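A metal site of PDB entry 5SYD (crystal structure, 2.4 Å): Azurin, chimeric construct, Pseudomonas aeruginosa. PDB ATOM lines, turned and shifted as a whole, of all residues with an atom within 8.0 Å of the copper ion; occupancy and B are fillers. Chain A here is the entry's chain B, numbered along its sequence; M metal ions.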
ATOM      1  N   VAL A   3     -27.109  10.225  10.002  1.00  0.00           N
ATOM      2  CA  VAL A   3     -26.086   9.175   9.946  1.00  0.00           C
ATOM      3  C   VAL A   3     -24.730   9.768   9.592  1.00  0.00           C
ATOM      4  O   VAL A   3     -23.699   9.231  10.007  1.00  0.00           O
ATOM      5  CB  VAL A   3     -26.495   8.052   8.964  1.00  0.00           C
ATOM      6  CG1 VAL A   3     -25.336   7.199   8.593  1.00  0.00           C
ATOM      7  CG2 VAL A   3     -27.575   7.219   9.568  1.00  0.00           C
ATOM      8  N   MET A   4     -24.696  10.899   8.888  1.00  0.00           N
ATOM      9  CA  MET A   4     -23.423  11.371   8.379  1.00  0.00           C
ATOM     10  C   MET A   4     -23.151  12.830   8.769  1.00  0.00           C
ATOM     11  O   MET A   4     -22.428  13.547   8.074  1.00  0.00           O
ATOM     12  CB  MET A   4     -23.336  11.171   6.867  1.00  0.00           C
ATOM     13  CG  MET A   4     -21.919  11.194   6.302  1.00  0.00           C
ATOM     14  SD  MET A   4     -20.855  10.072   7.239  1.00  0.00           S
ATOM     15  CE  MET A   4     -21.632   8.486   6.909  1.00  0.00           C
ATOM     16  N   GLY A   5     -23.710  13.288   9.885  1.00  0.00           N
ATOM     17  CA  GLY A   5     -23.325  14.582  10.397  1.00  0.00           C
ATOM     18  C   GLY A   5     -21.919  14.535  10.979  1.00  0.00           C
ATOM     19  O   GLY A   5     -21.454  13.502  11.445  1.00  0.00           O
ATOM     20  N   HIS A   6     -21.237  15.677  10.949  1.00  0.00           N
ATOM     21  CA  HIS A   6     -19.908  15.780  11.520  1.00  0.00           C
ATOM     22  C   HIS A   6     -19.789  17.025  12.397  1.00  0.00           C
ATOM     23  O   HIS A   6     -20.433  18.042  12.146  1.00  0.00           O
ATOM     24  CB  HIS A   6     -18.810  15.828  10.436  1.00  0.00           C
ATOM     25  CG  HIS A   6     -18.903  14.728   9.413  1.00  0.00           C
ATOM     26  ND1 HIS A   6     -18.771  13.398   9.739  1.00  0.00           N
ATOM     27  CD2 HIS A   6     -19.089  14.784   8.078  1.00  0.00           C
ATOM     28  CE1 HIS A   6     -18.882  12.665   8.642  1.00  0.00           C
ATOM     29  NE2 HIS A   6     -19.083  13.483   7.617  1.00  0.00           N
ATOM     30  N   ASN A   7     -18.939  16.917  13.421  1.00  0.00           N
ATOM     31  CA  ASN A   7     -18.479  18.057  14.195  1.00  0.00           C
ATOM     32  C   ASN A   7     -16.986  17.880  14.438  1.00  0.00           C
ATOM     33  O   ASN A   7     -16.386  16.874  14.038  1.00  0.00           O
ATOM     34  CB  ASN A   7     -19.240  18.236  15.514  1.00  0.00           C
ATOM     35  CG  ASN A   7     -19.091  17.048  16.472  1.00  0.00           C
ATOM     36  OD1 ASN A   7     -18.305  16.134  16.238  1.00  0.00           O
ATOM     37  ND2 ASN A   7     -19.828  17.087  17.569  1.00  0.00           N
ATOM     38  N   TRP A   8     -16.376  18.849  15.101  1.00  0.00           N
ATOM     39  CA  TRP A   8     -14.949  18.806  15.409  1.00  0.00           C
ATOM     40  C   TRP A   8     -14.788  19.131  16.888  1.00  0.00           C
ATOM     41  O   TRP A   8     -15.124  20.238  17.322  1.00  0.00           O
ATOM     42  CB  TRP A   8     -14.154  19.788  14.544  1.00  0.00           C
ATOM     43  CG  TRP A   8     -12.668  19.645  14.715  1.00  0.00           C
ATOM     44  CD1 TRP A   8     -11.838  18.855  13.976  1.00  0.00           C
ATOM     45  CD2 TRP A   8     -11.846  20.304  15.690  1.00  0.00           C
ATOM     46  NE1 TRP A   8     -10.543  18.974  14.437  1.00  0.00           N
ATOM     47  CE2 TRP A   8     -10.528  19.857  15.481  1.00  0.00           C
ATOM     48  CE3 TRP A   8     -12.101  21.219  16.711  1.00  0.00           C
ATOM     49  CZ2 TRP A   8      -9.455  20.309  16.260  1.00  0.00           C
ATOM     50  CZ3 TRP A   8     -11.037  21.664  17.482  1.00  0.00           C
ATOM     51  CH2 TRP A   8      -9.736  21.202  17.257  1.00  0.00           C
ATOM     52  N   LEU A  46     -22.451  20.735  14.916  1.00  0.00           N
ATOM     53  CA  LEU A  46     -22.638  19.608  14.023  1.00  0.00           C
ATOM     54  C   LEU A  46     -23.181  20.119  12.691  1.00  0.00           C
ATOM     55  O   LEU A  46     -24.151  20.875  12.667  1.00  0.00           O
ATOM     56  CB  LEU A  46     -23.582  18.606  14.689  1.00  0.00           C
ATOM     57  CG  LEU A  46     -23.615  17.118  14.390  1.00  0.00           C
ATOM     58  CD1 LEU A  46     -22.290  16.477  14.741  1.00  0.00           C
ATOM     59  CD2 LEU A  46     -24.689  16.521  15.283  1.00  0.00           C
ATOM     60  N   ILE A  47     -22.546  19.730  11.577  1.00  0.00           N
ATOM     61  CA  ILE A  47     -22.910  20.266  10.270  1.00  0.00           C
ATOM     62  C   ILE A  47     -23.240  19.136   9.304  1.00  0.00           C
ATOM     63  O   ILE A  47     -22.668  18.044   9.357  1.00  0.00           O
ATOM     64  CB  ILE A  47     -21.793  21.155   9.660  1.00  0.00           C
ATOM     65  CG1 ILE A  47     -20.534  20.340   9.377  1.00  0.00           C
ATOM     66  CG2 ILE A  47     -21.454  22.309  10.594  1.00  0.00           C
ATOM     67  CD1 ILE A  47     -19.477  21.111   8.618  1.00  0.00           C
ATOM     68  N   PHE A  71     -11.786  14.721  17.195  1.00  0.00           N
ATOM     69  CA  PHE A  71     -12.669  13.635  16.769  1.00  0.00           C
ATOM     70  C   PHE A  71     -14.070  14.196  16.536  1.00  0.00           C
ATOM     71  O   PHE A  71     -14.391  15.316  16.943  1.00  0.00           O
ATOM     72  CB  PHE A  71     -12.704  12.543  17.833  1.00  0.00           C
ATOM     73  CG  PHE A  71     -12.985  13.068  19.222  1.00  0.00           C
ATOM     74  CD1 PHE A  71     -11.956  13.446  20.054  1.00  0.00           C
ATOM     75  CD2 PHE A  71     -14.291  13.213  19.662  1.00  0.00           C
ATOM     76  CE1 PHE A  71     -12.215  13.948  21.314  1.00  0.00           C
ATOM     77  CE2 PHE A  71     -14.558  13.717  20.916  1.00  0.00           C
ATOM     78  CZ  PHE A  71     -13.509  14.081  21.752  1.00  0.00           C
ATOM     79  N   CYS A  72     -14.889  13.403  15.852  1.00  0.00           N
ATOM     80  CA  CYS A  72     -16.314  13.666  15.751  1.00  0.00           C
ATOM     81  C   CYS A  72     -17.073  12.826  16.770  1.00  0.00           C
ATOM     82  O   CYS A  72     -16.761  11.652  16.966  1.00  0.00           O
ATOM     83  CB  CYS A  72     -16.859  13.363  14.361  1.00  0.00           C
ATOM     84  SG  CYS A  72     -18.635  13.705  14.285  1.00  0.00           S
ATOM     85  N   THR A  73     -18.079  13.430  17.404  1.00  0.00           N
ATOM     86  CA  THR A  73     -18.874  12.759  18.435  1.00  0.00           C
ATOM     87  C   THR A  73     -20.178  12.180  17.903  1.00  0.00           C
ATOM     88  O   THR A  73     -20.920  11.566  18.676  1.00  0.00           O
ATOM     89  CB  THR A  73     -19.191  13.715  19.575  1.00  0.00           C
ATOM     90  OG1 THR A  73     -19.963  14.819  19.080  1.00  0.00           O
ATOM     91  CG2 THR A  73     -17.918  14.229  20.211  1.00  0.00           C
ATOM     92  N   PHE A  74     -20.490  12.362  16.620  1.00  0.00           N
ATOM     93  CA  PHE A  74     -21.668  11.736  16.052  1.00  0.00           C
ATOM     94  C   PHE A  74     -21.569  10.226  16.267  1.00  0.00           C
ATOM     95  O   PHE A  74     -20.509   9.642  15.987  1.00  0.00           O
ATOM     96  CB  PHE A  74     -21.806  12.078  14.567  1.00  0.00           C
ATOM     97  CG  PHE A  74     -23.152  11.755  13.977  1.00  0.00           C
ATOM     98  CD1 PHE A  74     -23.481  10.451  13.633  1.00  0.00           C
ATOM     99  CD2 PHE A  74     -24.083  12.754  13.766  1.00  0.00           C
ATOM    100  CE1 PHE A  74     -24.730  10.164  13.089  1.00  0.00           C
ATOM    101  CE2 PHE A  74     -25.317  12.474  13.222  1.00  0.00           C
ATOM    102  CZ  PHE A  74     -25.639  11.168  12.885  1.00  0.00           C
ATOM    103  N   PRO A  75     -22.620   9.569  16.780  1.00  0.00           N
ATOM    104  CA  PRO A  75     -22.495   8.176  17.233  1.00  0.00           C
ATOM    105  C   PRO A  75     -21.810   7.238  16.257  1.00  0.00           C
ATOM    106  O   PRO A  75     -22.262   7.070  15.111  1.00  0.00           O
ATOM    107  CB  PRO A  75     -23.949   7.746  17.464  1.00  0.00           C
ATOM    108  CG  PRO A  75     -24.654   9.018  17.804  1.00  0.00           C
ATOM    109  CD  PRO A  75     -23.976  10.095  16.985  1.00  0.00           C
ATOM    110  N   GLY A  76     -20.719   6.613  16.696  1.00  0.00           N
ATOM    111  CA  GLY A  76     -19.983   5.674  15.899  1.00  0.00           C
ATOM    112  C   GLY A  76     -18.869   6.263  15.066  1.00  0.00           C
ATOM    113  O   GLY A  76     -17.977   5.520  14.636  1.00  0.00           O
ATOM    114  N   HIS A  77     -18.890   7.571  14.809  1.00  0.00           N
ATOM    115  CA  HIS A  77     -17.958   8.162  13.857  1.00  0.00           C
ATOM    116  C   HIS A  77     -16.523   8.236  14.373  1.00  0.00           C
ATOM    117  O   HIS A  77     -15.581   8.145  13.588  1.00  0.00           O
ATOM    118  CB  HIS A  77     -18.462   9.544  13.444  1.00  0.00           C
ATOM    119  CG  HIS A  77     -19.676   9.504  12.576  1.00  0.00           C
ATOM    120  ND1 HIS A  77     -19.994  10.503  11.692  1.00  0.00           N
ATOM    121  CD2 HIS A  77     -20.658   8.578  12.452  1.00  0.00           C
ATOM    122  CE1 HIS A  77     -21.115  10.209  11.060  1.00  0.00           C
ATOM    123  NE2 HIS A  77     -21.537   9.040  11.503  1.00  0.00           N
ATOM    124  N   SER A  78     -16.329   8.408  15.693  1.00  0.00           N
ATOM    125  CA  SER A  78     -14.966   8.566  16.214  1.00  0.00           C
ATOM    126  C   SER A  78     -14.073   7.364  15.921  1.00  0.00           C
ATOM    127  O   SER A  78     -12.851   7.473  16.052  1.00  0.00           O
ATOM    128  CB  SER A  78     -14.986   8.826  17.720  1.00  0.00           C
ATOM    129  OG  SER A  78     -15.796   7.891  18.399  1.00  0.00           O
ATOM    130  N   MET A  81     -13.011   8.763  12.571  1.00  0.00           N
ATOM    131  CA  MET A  81     -12.907  10.220  12.573  1.00  0.00           C
ATOM    132  C   MET A  81     -12.258  10.676  13.872  1.00  0.00           C
ATOM    133  O   MET A  81     -12.892  11.213  14.791  1.00  0.00           O
ATOM    134  CB  MET A  81     -14.274  10.841  12.371  1.00  0.00           C
ATOM    135  CG  MET A  81     -14.803  10.640  10.970  1.00  0.00           C
ATOM    136  SD  MET A  81     -16.334  11.536  10.669  1.00  0.00           S
ATOM    137  CE  MET A  81     -15.622  13.073  10.129  1.00  0.00           C
ATOM    138  N   GLY A 102     -14.932  16.720   6.753  1.00  0.00           N
ATOM    139  CA  GLY A 102     -15.508  15.395   6.951  1.00  0.00           C
ATOM    140  C   GLY A 102     -16.354  15.050   5.748  1.00  0.00           C
ATOM    141  O   GLY A 102     -17.135  15.875   5.266  1.00  0.00           O
ATOM    142  N   ASN A 103     -16.195  13.821   5.249  1.00  0.00           N
ATOM    143  CA  ASN A 103     -16.790  13.465   3.974  1.00  0.00           C
ATOM    144  C   ASN A 103     -17.992  12.535   4.148  1.00  0.00           C
ATOM    145  O   ASN A 103     -18.506  12.358   5.251  1.00  0.00           O
ATOM    146  CB  ASN A 103     -15.731  12.842   3.053  1.00  0.00           C
ATOM    147  CG  ASN A 103     -15.184  11.534   3.586  1.00  0.00           C
ATOM    148  OD1 ASN A 103     -15.560  11.067   4.670  1.00  0.00           O
ATOM    149  ND2 ASN A 103     -14.299  10.914   2.819  1.00  0.00           N
ATOM    150  N   MET A 106     -17.532   8.923   6.406  1.00  0.00           N
ATOM    151  CA  MET A 106     -17.128   8.929   7.813  1.00  0.00           C
ATOM    152  C   MET A 106     -15.618   9.102   7.985  1.00  0.00           C
ATOM    153  O   MET A 106     -14.980   8.394   8.770  1.00  0.00           O
ATOM    154  CB  MET A 106     -17.604   7.652   8.512  1.00  0.00           C
ATOM    155  CG  MET A 106     -18.118   7.841   9.929  1.00  0.00           C
ATOM    156  SD  MET A 106     -18.809   6.317  10.607  1.00  0.00           S
ATOM    157  CE  MET A 106     -17.325   5.328  10.784  1.00  0.00           C
ATOM    158  N   GLN A 107     -15.036  10.039   7.238  1.00  0.00           N
ATOM    159  CA  GLN A 107     -13.609  10.301   7.286  1.00  0.00           C
ATOM    160  C   GLN A 107     -13.318  11.799   7.387  1.00  0.00           C
ATOM    161  O   GLN A 107     -13.938  12.610   6.700  1.00  0.00           O
ATOM    162  CB  GLN A 107     -12.905   9.734   6.056  1.00  0.00           C
ATOM    163  CG  GLN A 107     -12.771   8.222   6.074  1.00  0.00           C
ATOM    164  CD  GLN A 107     -12.172   7.691   4.805  1.00  0.00           C
ATOM    165  OE1 GLN A 107     -12.470   8.179   3.702  1.00  0.00           O
ATOM    166  NE2 GLN A 107     -11.315   6.681   4.924  1.00  0.00           N
ATOM    167  N   PHE A 108     -12.369  12.154   8.255  1.00  0.00           N
ATOM    168  CA  PHE A 108     -11.674  13.434   8.187  1.00  0.00           C
ATOM    169  C   PHE A 108     -10.561  13.339   7.139  1.00  0.00           C
ATOM    170  O   PHE A 108     -10.068  12.254   6.831  1.00  0.00           O
ATOM    171  CB  PHE A 108     -11.090  13.818   9.547  1.00  0.00           C
ATOM    172  CG  PHE A 108     -12.080  14.444  10.501  1.00  0.00           C
ATOM    173  CD1 PHE A 108     -12.961  15.423  10.067  1.00  0.00           C
ATOM    174  CD2 PHE A 108     -12.122  14.050  11.827  1.00  0.00           C
ATOM    175  CE1 PHE A 108     -13.857  16.002  10.957  1.00  0.00           C
ATOM    176  CE2 PHE A 108     -13.013  14.620  12.707  1.00  0.00           C
ATOM    177  CZ  PHE A 108     -13.887  15.595  12.280  1.00  0.00           C
ATOM    178  N   LEU A 126     -14.226  23.833   9.761  1.00  0.00           N
ATOM    179  CA  LEU A 126     -14.805  22.565   9.358  1.00  0.00           C
ATOM    180  C   LEU A 126     -15.791  22.781   8.217  1.00  0.00           C
ATOM    181  O   LEU A 126     -16.638  23.673   8.291  1.00  0.00           O
ATOM    182  CB  LEU A 126     -15.502  21.890  10.542  1.00  0.00           C
ATOM    183  CG  LEU A 126     -16.150  20.540  10.264  1.00  0.00           C
ATOM    184  CD1 LEU A 126     -15.106  19.446  10.026  1.00  0.00           C
ATOM    185  CD2 LEU A 126     -17.098  20.157  11.393  1.00  0.00           C
ATOM    186  N   HIS A 128     -18.125  20.249   5.101  1.00  0.00           N
ATOM    187  CA  HIS A 128     -18.636  18.925   4.771  1.00  0.00           C
ATOM    188  C   HIS A 128     -19.099  18.939   3.313  1.00  0.00           C
ATOM    189  O   HIS A 128     -20.299  18.959   3.018  1.00  0.00           O
ATOM    190  CB  HIS A 128     -19.785  18.551   5.710  1.00  0.00           C
ATOM    191  CG  HIS A 128     -20.296  17.144   5.551  1.00  0.00           C
ATOM    192  ND1 HIS A 128     -19.935  16.330   4.493  1.00  0.00           N
ATOM    193  CD2 HIS A 128     -21.166  16.425   6.289  1.00  0.00           C
ATOM    194  CE1 HIS A 128     -20.547  15.171   4.609  1.00  0.00           C
ATOM    195  NE2 HIS A 128     -21.303  15.195   5.690  1.00  0.00           N
HETATM  196 CU    CU M   1     -18.859  12.619  11.989  1.00  0.00          CU
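O of His 6 lies within hydrogen-bond range of N of Ile 47 (2.8 Å).
A ring nitrogen (NE2) of His 6 sits at hydrogen-bond distance from the backbone carbonyl oxygen (O) of Met 4.
A ring nitrogen (NE2) of His 6 is in hydrogen-bond range of the backbone carbonyl oxygen (O) of Asn 103 (2.7 Å).
A ring nitrogen (ND1) of His 77 lies close to the backbone carbonyl oxygen of Gly 5 (3.3 Å).
N of Phe 74 lies close to SG of Cys 72 (3.3 Å).
ND1 of His 6 sits close to SD of Met 81.
The backbone NH (N) of Cys 72 lies within hydrogen-bond range of the backbone carbonyl oxygen (O) of Met 81, 3.1 Å away.
A ring nitrogen (NE2) of His 6 lies close to a ring nitrogen (NE2) of His 128 (3.4 Å).
Residues that only touch the copper ion: Phe 74.
Within 4 Å of the copper ion: Gly 5, His 6, Cys 72, Phe 74, His 77 and Met 81.
Along chain A the residues within 4 Å of the copper ion span positions 5 to 81.
The nearest printed residue that does not touch the copper ion is Asn 7 (4.5 Å).
The copper ion is bound by a ring nitrogen (ND1) of His 6 (2.4 Å), a ring nitrogen (ND1) of His 77 (2.4 Å) and the side-chain sulfur (SG) of Cys 72 (2.5 Å).
The copper ion has three donor atoms within binding distance.
Slightly farther from the copper ion lies the backbone carbonyl oxygen (O) of Gly 5 (2.8 Å).
Slightly farther from the copper ion lies the side-chain sulfur (SD) of Met 81 (3.0 Å).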
